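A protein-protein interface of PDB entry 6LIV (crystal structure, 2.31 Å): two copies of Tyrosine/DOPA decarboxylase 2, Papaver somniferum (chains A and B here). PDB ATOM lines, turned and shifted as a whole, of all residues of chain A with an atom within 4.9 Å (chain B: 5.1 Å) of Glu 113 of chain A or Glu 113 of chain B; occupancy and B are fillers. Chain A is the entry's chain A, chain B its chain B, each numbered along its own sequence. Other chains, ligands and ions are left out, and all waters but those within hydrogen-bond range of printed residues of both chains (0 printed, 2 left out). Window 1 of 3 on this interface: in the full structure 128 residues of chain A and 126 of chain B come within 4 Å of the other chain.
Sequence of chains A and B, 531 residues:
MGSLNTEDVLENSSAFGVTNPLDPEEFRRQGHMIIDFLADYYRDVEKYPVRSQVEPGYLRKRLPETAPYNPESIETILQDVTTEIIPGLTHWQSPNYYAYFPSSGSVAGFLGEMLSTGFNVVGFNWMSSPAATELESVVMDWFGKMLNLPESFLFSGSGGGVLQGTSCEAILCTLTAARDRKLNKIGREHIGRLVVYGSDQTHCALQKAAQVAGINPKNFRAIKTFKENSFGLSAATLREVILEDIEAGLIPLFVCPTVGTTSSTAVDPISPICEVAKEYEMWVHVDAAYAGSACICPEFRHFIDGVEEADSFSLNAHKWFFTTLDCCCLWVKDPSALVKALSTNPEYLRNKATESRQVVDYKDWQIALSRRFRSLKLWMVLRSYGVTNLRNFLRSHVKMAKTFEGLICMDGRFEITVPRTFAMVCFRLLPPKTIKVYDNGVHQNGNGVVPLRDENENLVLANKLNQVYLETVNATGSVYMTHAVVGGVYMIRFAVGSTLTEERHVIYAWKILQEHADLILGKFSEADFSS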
ATOM      1  N   GLY A 109      -1.224  -9.983  10.242  1.00  0.00           N
ATOM      2  CA  GLY A 109      -0.189 -10.203   9.251  1.00  0.00           C
ATOM      3  C   GLY A 109       1.210  -9.990   9.798  1.00  0.00           C
ATOM      4  O   GLY A 109       2.143 -10.708   9.431  1.00  0.00           O
ATOM      5  N   PHE A 110       1.381  -8.988  10.666  1.00  0.00           N
ATOM      6  CA  PHE A 110       2.665  -8.808  11.334  1.00  0.00           C
ATOM      7  C   PHE A 110       3.034 -10.045  12.140  1.00  0.00           C
ATOM      8  O   PHE A 110       4.182 -10.504  12.101  1.00  0.00           O
ATOM      9  CB  PHE A 110       2.626  -7.572  12.236  1.00  0.00           C
ATOM     10  CG  PHE A 110       3.859  -7.396  13.086  1.00  0.00           C
ATOM     11  CD1 PHE A 110       3.930  -7.949  14.358  1.00  0.00           C
ATOM     12  CD2 PHE A 110       4.942  -6.671  12.617  1.00  0.00           C
ATOM     13  CE1 PHE A 110       5.060  -7.789  15.139  1.00  0.00           C
ATOM     14  CE2 PHE A 110       6.074  -6.506  13.395  1.00  0.00           C
ATOM     15  CZ  PHE A 110       6.133  -7.065  14.657  1.00  0.00           C
ATOM     16  N   LEU A 111       2.071 -10.598  12.881  1.00  0.00           N
ATOM     17  CA  LEU A 111       2.338 -11.788  13.680  1.00  0.00           C
ATOM     18  C   LEU A 111       2.665 -12.991  12.805  1.00  0.00           C
ATOM     19  O   LEU A 111       3.452 -13.854  13.212  1.00  0.00           O
ATOM     20  CB  LEU A 111       1.143 -12.096  14.579  1.00  0.00           C
ATOM     21  CG  LEU A 111       0.680 -11.011  15.553  1.00  0.00           C
ATOM     22  CD1 LEU A 111      -0.611 -11.435  16.229  1.00  0.00           C
ATOM     23  CD2 LEU A 111       1.754 -10.704  16.584  1.00  0.00           C
ATOM     24  N   GLY A 112       2.069 -13.074  11.613  1.00  0.00           N
ATOM     25  CA  GLY A 112       2.421 -14.149  10.699  1.00  0.00           C
ATOM     26  C   GLY A 112       3.876 -14.091  10.278  1.00  0.00           C
ATOM     27  O   GLY A 112       4.574 -15.109  10.262  1.00  0.00           O
ATOM     28  N   GLU A 113       4.354 -12.892   9.933  1.00  0.00           N
ATOM     29  CA  GLU A 113       5.769 -12.718   9.618  1.00  0.00           C
ATOM     30  C   GLU A 113       6.640 -13.012  10.832  1.00  0.00           C
ATOM     31  O   GLU A 113       7.739 -13.563  10.701  1.00  0.00           O
ATOM     32  CB  GLU A 113       6.027 -11.295   9.118  1.00  0.00           C
ATOM     33  CG  GLU A 113       6.254 -11.183   7.621  1.00  0.00           C
ATOM     34  CD  GLU A 113       7.449 -11.982   7.144  1.00  0.00           C
ATOM     35  OE1 GLU A 113       8.588 -11.486   7.272  1.00  0.00           O
ATOM     36  OE2 GLU A 113       7.249 -13.107   6.638  1.00  0.00           O
ATOM     37  N   MET A 114       6.163 -12.645  12.023  1.00  0.00           N
ATOM     38  CA  MET A 114       6.918 -12.898  13.245  1.00  0.00           C
ATOM     39  C   MET A 114       7.125 -14.392  13.461  1.00  0.00           C
ATOM     40  O   MET A 114       8.244 -14.845  13.732  1.00  0.00           O
ATOM     41  CB  MET A 114       6.191 -12.271  14.435  1.00  0.00           C
ATOM     42  CG  MET A 114       7.042 -12.100  15.674  1.00  0.00           C
ATOM     43  SD  MET A 114       6.314 -10.945  16.852  1.00  0.00           S
ATOM     44  CE  MET A 114       7.592  -9.698  16.941  1.00  0.00           C
ATOM     45  N   LEU A 115       6.049 -15.175  13.346  1.00  0.00           N
ATOM     46  CA  LEU A 115       6.168 -16.624  13.474  1.00  0.00           C
ATOM     47  C   LEU A 115       7.035 -17.205  12.363  1.00  0.00           C
ATOM     48  O   LEU A 115       7.798 -18.150  12.591  1.00  0.00           O
ATOM     49  CB  LEU A 115       4.782 -17.266  13.464  1.00  0.00           C
ATOM     50  CG  LEU A 115       3.920 -17.056  14.709  1.00  0.00           C
ATOM     51  CD1 LEU A 115       2.500 -17.543  14.467  1.00  0.00           C
ATOM     52  CD2 LEU A 115       4.534 -17.758  15.909  1.00  0.00           C
ATOM     53  N   SER A 116       6.927 -16.653  11.153  1.00  0.00           N
ATOM     54  CA  SER A 116       7.752 -17.125  10.046  1.00  0.00           C
ATOM     55  C   SER A 116       9.225 -16.831  10.298  1.00  0.00           C
ATOM     56  O   SER A 116      10.083 -17.707  10.126  1.00  0.00           O
ATOM     57  CB  SER A 116       7.286 -16.486   8.737  1.00  0.00           C
ATOM     58  OG  SER A 116       8.201 -16.746   7.687  1.00  0.00           O
ATOM     59  N   THR A 117       9.538 -15.601  10.711  1.00  0.00           N
ATOM     60  CA  THR A 117      10.917 -15.260  11.044  1.00  0.00           C
ATOM     61  C   THR A 117      11.385 -15.987  12.299  1.00  0.00           C
ATOM     62  O   THR A 117      12.579 -16.286  12.433  1.00  0.00           O
ATOM     63  CB  THR A 117      11.051 -13.746  11.219  1.00  0.00           C
ATOM     64  OG1 THR A 117      10.426 -13.080  10.117  1.00  0.00           O
ATOM     65  CG2 THR A 117      12.512 -13.338  11.283  1.00  0.00           C
ATOM     66  N   GLY A 118      10.467 -16.289  13.219  1.00  0.00           N
ATOM     67  CA  GLY A 118      10.851 -17.001  14.427  1.00  0.00           C
ATOM     68  C   GLY A 118      11.218 -18.447  14.154  1.00  0.00           C
ATOM     69  O   GLY A 118      12.290 -18.914  14.549  1.00  0.00           O
ATOM     70  N   THR A 324       1.513  -8.244   4.888  1.00  0.00           N
ATOM     71  CA  THR A 324       2.437  -7.152   5.157  1.00  0.00           C
ATOM     72  C   THR A 324       3.366  -7.246   3.960  1.00  0.00           C
ATOM     73  O   THR A 324       3.267  -8.223   3.213  1.00  0.00           O
ATOM     74  CB  THR A 324       3.148  -7.275   6.509  1.00  0.00           C
ATOM     75  OG1 THR A 324       3.543  -5.974   6.967  1.00  0.00           O
ATOM     76  CG2 THR A 324       4.350  -8.181   6.406  1.00  0.00           C
ATOM     77  N   ARG A 372      10.468 -18.641   1.778  1.00  0.00           N
ATOM     78  CA  ARG A 372      10.045 -18.211   3.099  1.00  0.00           C
ATOM     79  C   ARG A 372       8.654 -18.746   3.414  1.00  0.00           C
ATOM     80  O   ARG A 372       7.847 -19.006   2.518  1.00  0.00           O
ATOM     81  CB  ARG A 372      10.052 -16.683   3.204  1.00  0.00           C
ATOM     82  CG  ARG A 372      11.431 -16.052   3.084  1.00  0.00           C
ATOM     83  CD  ARG A 372      11.406 -14.579   3.464  1.00  0.00           C
ATOM     84  NE  ARG A 372      11.090 -14.379   4.877  1.00  0.00           N
ATOM     85  CZ  ARG A 372      11.215 -13.219   5.513  1.00  0.00           C
ATOM     86  NH1 ARG A 372      11.652 -12.147   4.865  1.00  0.00           N
ATOM     87  NH2 ARG A 372      10.904 -13.129   6.800  1.00  0.00           N
ATOM     88  N   LYS A 377       1.428 -15.540   7.132  1.00  0.00           N
ATOM     89  CA  LYS A 377       0.824 -14.215   7.015  1.00  0.00           C
ATOM     90  C   LYS A 377      -0.613 -14.301   6.516  1.00  0.00           C
ATOM     91  O   LYS A 377      -1.547 -13.820   7.169  1.00  0.00           O
ATOM     92  CB  LYS A 377       1.648 -13.347   6.062  1.00  0.00           C
ATOM     93  CG  LYS A 377       2.874 -12.700   6.660  1.00  0.00           C
ATOM     94  CD  LYS A 377       3.463 -11.717   5.664  1.00  0.00           C
ATOM     95  CE  LYS A 377       4.209 -12.438   4.554  1.00  0.00           C
ATOM     96  NZ  LYS A 377       5.381 -11.654   4.073  1.00  0.00           N
ATOM     97  N   ALA B 108      19.231 -10.424  17.116  1.00  0.00           N
ATOM     98  CA  ALA B 108      19.383  -9.156  16.407  1.00  0.00           C
ATOM     99  C   ALA B 108      18.771  -9.217  15.014  1.00  0.00           C
ATOM    100  O   ALA B 108      18.074  -8.286  14.594  1.00  0.00           O
ATOM    101  CB  ALA B 108      20.862  -8.777  16.328  1.00  0.00           C
ATOM    102  N   GLY B 109      19.021 -10.304  14.280  1.00  0.00           N
ATOM    103  CA  GLY B 109      18.420 -10.445  12.963  1.00  0.00           C
ATOM    104  C   GLY B 109      16.905 -10.483  13.017  1.00  0.00           C
ATOM    105  O   GLY B 109      16.228  -9.912  12.159  1.00  0.00           O
ATOM    106  N   PHE B 110      16.354 -11.156  14.031  1.00  0.00           N
ATOM    107  CA  PHE B 110      14.904 -11.214  14.184  1.00  0.00           C
ATOM    108  C   PHE B 110      14.321  -9.831  14.453  1.00  0.00           C
ATOM    109  O   PHE B 110      13.300  -9.457  13.864  1.00  0.00           O
ATOM    110  CB  PHE B 110      14.541 -12.184  15.309  1.00  0.00           C
ATOM    111  CG  PHE B 110      13.074 -12.225  15.633  1.00  0.00           C
ATOM    112  CD1 PHE B 110      12.542 -11.400  16.612  1.00  0.00           C
ATOM    113  CD2 PHE B 110      12.230 -13.095  14.967  1.00  0.00           C
ATOM    114  CE1 PHE B 110      11.197 -11.437  16.912  1.00  0.00           C
ATOM    115  CE2 PHE B 110      10.883 -13.138  15.265  1.00  0.00           C
ATOM    116  CZ  PHE B 110      10.368 -12.308  16.240  1.00  0.00           C
ATOM    117  N   LEU B 111      14.952  -9.062  15.343  1.00  0.00           N
ATOM    118  CA  LEU B 111      14.451  -7.726  15.653  1.00  0.00           C
ATOM    119  C   LEU B 111      14.537  -6.807  14.442  1.00  0.00           C
ATOM    120  O   LEU B 111      13.640  -5.986  14.216  1.00  0.00           O
ATOM    121  CB  LEU B 111      15.225  -7.127  16.827  1.00  0.00           C
ATOM    122  CG  LEU B 111      15.357  -7.948  18.110  1.00  0.00           C
ATOM    123  CD1 LEU B 111      16.165  -7.173  19.134  1.00  0.00           C
ATOM    124  CD2 LEU B 111      13.997  -8.330  18.669  1.00  0.00           C
ATOM    125  N   GLY B 112      15.610  -6.924  13.657  1.00  0.00           N
ATOM    126  CA  GLY B 112      15.724  -6.110  12.458  1.00  0.00           C
ATOM    127  C   GLY B 112      14.630  -6.405  11.451  1.00  0.00           C
ATOM    128  O   GLY B 112      14.153  -5.505  10.756  1.00  0.00           O
ATOM    129  N   GLU B 113      14.215  -7.671  11.360  1.00  0.00           N
ATOM    130  CA  GLU B 113      13.118  -8.018  10.466  1.00  0.00           C
ATOM    131  C   GLU B 113      11.778  -7.540  11.010  1.00  0.00           C
ATOM    132  O   GLU B 113      10.900  -7.145  10.233  1.00  0.00           O
ATOM    133  CB  GLU B 113      13.092  -9.529  10.228  1.00  0.00           C
ATOM    134  CG  GLU B 113      11.974 -10.004   9.304  1.00  0.00           C
ATOM    135  CD  GLU B 113      12.250  -9.721   7.835  1.00  0.00           C
ATOM    136  OE1 GLU B 113      13.201  -8.969   7.528  1.00  0.00           O
ATOM    137  OE2 GLU B 113      11.509 -10.255   6.982  1.00  0.00           O
ATOM    138  N   MET B 114      11.603  -7.558  12.333  1.00  0.00           N
ATOM    139  CA  MET B 114      10.347  -7.091  12.909  1.00  0.00           C
ATOM    140  C   MET B 114      10.230  -5.575  12.843  1.00  0.00           C
ATOM    141  O   MET B 114       9.125  -5.048  12.665  1.00  0.00           O
ATOM    142  CB  MET B 114      10.217  -7.588  14.345  1.00  0.00           C
ATOM    143  CG  MET B 114      10.012  -9.092  14.438  1.00  0.00           C
ATOM    144  SD  MET B 114       8.557  -9.646  13.520  1.00  0.00           S
ATOM    145  CE  MET B 114       9.303 -10.368  12.059  1.00  0.00           C
ATOM    146  N   LEU B 115      11.347  -4.860  12.989  1.00  0.00           N
ATOM    147  CA  LEU B 115      11.335  -3.427  12.718  1.00  0.00           C
ATOM    148  C   LEU B 115      11.038  -3.161  11.248  1.00  0.00           C
ATOM    149  O   LEU B 115      10.293  -2.233  10.914  1.00  0.00           O
ATOM    150  CB  LEU B 115      12.671  -2.801  13.118  1.00  0.00           C
ATOM    151  CG  LEU B 115      12.893  -2.572  14.614  1.00  0.00           C
ATOM    152  CD1 LEU B 115      14.268  -1.978  14.876  1.00  0.00           C
ATOM    153  CD2 LEU B 115      11.803  -1.681  15.185  1.00  0.00           C
ATOM    154  N   SER B 116      11.613  -3.968  10.354  1.00  0.00           N
ATOM    155  CA  SER B 116      11.291  -3.851   8.935  1.00  0.00           C
ATOM    156  C   SER B 116       9.818  -4.138   8.680  1.00  0.00           C
ATOM    157  O   SER B 116       9.152  -3.400   7.942  1.00  0.00           O
ATOM    158  CB  SER B 116      12.177  -4.797   8.124  1.00  0.00           C
ATOM    159  OG  SER B 116      11.798  -4.812   6.759  1.00  0.00           O
ATOM    160  N   THR B 117       9.289  -5.198   9.297  1.00  0.00           N
ATOM    161  CA  THR B 117       7.878  -5.526   9.135  1.00  0.00           C
ATOM    162  C   THR B 117       6.975  -4.524   9.853  1.00  0.00           C
ATOM    163  O   THR B 117       5.836  -4.303   9.427  1.00  0.00           O
ATOM    164  CB  THR B 117       7.625  -6.946   9.638  1.00  0.00           C
ATOM    165  OG1 THR B 117       8.526  -7.842   8.981  1.00  0.00           O
ATOM    166  CG2 THR B 117       6.195  -7.385   9.349  1.00  0.00           C
ATOM    167  N   GLY B 118       7.466  -3.900  10.927  1.00  0.00           N
ATOM    168  CA  GLY B 118       6.656  -2.927  11.646  1.00  0.00           C
ATOM    169  C   GLY B 118       6.507  -1.621  10.891  1.00  0.00           C
ATOM    170  O   GLY B 118       5.408  -1.068  10.791  1.00  0.00           O
ATOM    171  N   THR B 324      18.689 -14.088   9.617  1.00  0.00           N
ATOM    172  CA  THR B 324      17.406 -14.814   9.427  1.00  0.00           C
ATOM    173  C   THR B 324      17.024 -14.709   7.939  1.00  0.00           C
ATOM    174  O   THR B 324      17.449 -13.814   7.220  1.00  0.00           O
ATOM    175  CB  THR B 324      16.208 -14.535  10.393  1.00  0.00           C
ATOM    176  OG1 THR B 324      15.725 -13.201  10.204  1.00  0.00           O
ATOM    177  CG2 THR B 324      16.610 -14.720  11.839  1.00  0.00           C
ATOM    178  N   LEU B 325      16.230 -15.644   7.471  1.00  0.00           N
ATOM    179  CA  LEU B 325      15.867 -15.668   6.083  1.00  0.00           C
ATOM    180  C   LEU B 325      14.904 -14.538   5.750  1.00  0.00           C
ATOM    181  O   LEU B 325      13.955 -14.356   6.440  1.00  0.00           O
ATOM    182  CB  LEU B 325      15.255 -17.017   5.781  1.00  0.00           C
ATOM    183  CG  LEU B 325      14.849 -17.403   4.378  1.00  0.00           C
ATOM    184  CD1 LEU B 325      16.060 -17.721   3.544  1.00  0.00           C
ATOM    185  CD2 LEU B 325      13.910 -18.583   4.445  1.00  0.00           C
ATOM    186  N   ARG B 372      12.011  -4.706   0.265  1.00  0.00           N
ATOM    187  CA  ARG B 372      11.843  -4.691   1.708  1.00  0.00           C
ATOM    188  C   ARG B 372      13.035  -4.009   2.373  1.00  0.00           C
ATOM    189  O   ARG B 372      14.128  -3.915   1.807  1.00  0.00           O
ATOM    190  CB  ARG B 372      11.681  -6.113   2.251  1.00  0.00           C
ATOM    191  CG  ARG B 372      10.484  -6.868   1.691  1.00  0.00           C
ATOM    192  CD  ARG B 372      10.254  -8.175   2.437  1.00  0.00           C
ATOM    193  NE  ARG B 372       9.954  -7.954   3.850  1.00  0.00           N
ATOM    194  CZ  ARG B 372       9.580  -8.911   4.694  1.00  0.00           C
ATOM    195  NH1 ARG B 372       9.457 -10.161   4.271  1.00  0.00           N
ATOM    196  NH2 ARG B 372       9.327  -8.617   5.962  1.00  0.00           N
ATOM    197  N   LYS B 377      18.082  -5.784   9.252  1.00  0.00           N
ATOM    198  CA  LYS B 377      18.601  -7.070   9.714  1.00  0.00           C
ATOM    199  C   LYS B 377      20.121  -7.055   9.801  1.00  0.00           C
ATOM    200  O   LYS B 377      20.702  -7.378  10.843  1.00  0.00           O
ATOM    201  CB  LYS B 377      18.142  -8.187   8.778  1.00  0.00           C
ATOM    202  CG  LYS B 377      16.818  -8.824   9.143  1.00  0.00           C
ATOM    203  CD  LYS B 377      16.498  -9.966   8.196  1.00  0.00           C
ATOM    204  CE  LYS B 377      16.621  -9.529   6.745  1.00  0.00           C
ATOM    205  NZ  LYS B 377      15.668 -10.252   5.858  1.00  0.00           N
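OE1 of Glu 113 of chain A sits close to OE2 of Glu 113 of chain B.
NH1 of Arg 372 of chain A lies within salt-bridge range of OE2 of Glu 113 of chain B (2.8 Å).
The side-chain carboxylate of Glu 113 of chain A lies within salt-bridge range of the guanidinium group of Arg 372 of chain B.
NE of Arg 372 of chain A sits close to O of Leu 325 of chain B.
The guanidinium group (NH1) of Arg 372 of chain A lies close to the guanidinium group (NH1) of Arg 372 of chain B, at 3.0 Å.
O of Glu 113 of chain A lies within hydrogen-bond range of OG1 of Thr 117 of chain A (2.8 Å).
OG1 of Thr 117 of chain B lies within hydrogen-bond range of O of Glu 113 of chain B, 2.8 Å away.
OG1 of Thr 117 of chain B sits at hydrogen-bond distance from NH2 of Arg 372 of chain B (3.2 Å).
The guanidinium group (NH2) of Arg 372 of chain A lies within salt-bridge range of the side-chain carboxylate (OE1) of Glu 113 of chain A, 2.9 Å away.
OE2 of Glu 113 of chain A is in salt-bridge range of NZ of Lys 377 of chain A, at 3.5 Å.
The side-chain amino group of Lys 377 of chain B lies within salt-bridge range of the side-chain carboxylate of Glu 113 of chain B, at 3.2 Å.
Among the printed residues, pairs that only touch across the chains: Met 114 of chain A with Phe 110 of chain B, Thr 117 of chain A with Thr 324 of chain B, Phe 110 of chain A with Met 114 of chain B, Thr 117 of chain A with Met 114 of chain B, Met 114 of chain A with Met 114 of chain B, Thr 117 of chain A with Glu 113 of chain B, Thr 324 of chain A with Thr 117 of chain B, Phe 110 of chain A with Thr 117 of chain B, Thr 117 of chain A with Phe 110 of chain B, Gly 118 of chain A with Phe 110 of chain B, Glu 113 of chain A with Met 114 of chain B, Phe 110 of chain A with Gly 118 of chain B and Glu 113 of chain A with Thr 117 of chain B.
Leu 111 of chain A touches none of the printed residues of chain B.
Gly 112 of chain A touches none of the printed residues of chain B.
Glu 113 of chain A touches just these residues of chain B: Glu 113, Met 114, Thr 117 and Arg 372.
Of the printed residues of chain B, Arg 372 of chain A touches Glu 113, Leu 325 and Arg 372.
Of the printed residues of chain A, Met 114 of chain B touches Phe 110 (3.5 Å), Glu 113 (3.8 Å), Met 114 (3.5 Å) and Thr 117 (3.5 Å).
Of the printed residues of chain A, Leu 325 of chain B touches Arg 372 (3.1 Å).
Of the 13 printed residues of chain A, 7 touch a printed residue of chain B.
Printed residues of chain A that touch a printed residue of chain B: Phe 110, Glu 113, Met 114, Thr 117, Gly 118, Thr 324 and Arg 372.
Hydrophobic or aromatic side chains of chain A that line the printed part of chain B: Phe 110 and Met 114.
Of the 15 printed residues of chain B, 8 touch a printed residue of chain A.
Among the printed residues, 18 pairs touch across the chains.
Glu 113 of chain A touches Met 114 of chain B, but with the chains exchanged Met 114 of chain A does not touch Glu 113 of chain B (6.9 Å).
Thr 117 of chain A touches Met 114 of chain B, but with the chains exchanged Met 114 of chain A does not touch Thr 117 of chain B (5.9 Å).
Thr 117 of chain A touches Thr 324 of chain B, and with the chains exchanged Thr 324 of chain A touches Thr 117 of chain B.
Arg 372 of chain A touches its own counterpart, Arg 372 of chain B.
13 positions are printed for both chains.
Of the 18 pairs that touch across the chains among the printed residues, 15 have their exchanged pair printed and touching as well.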
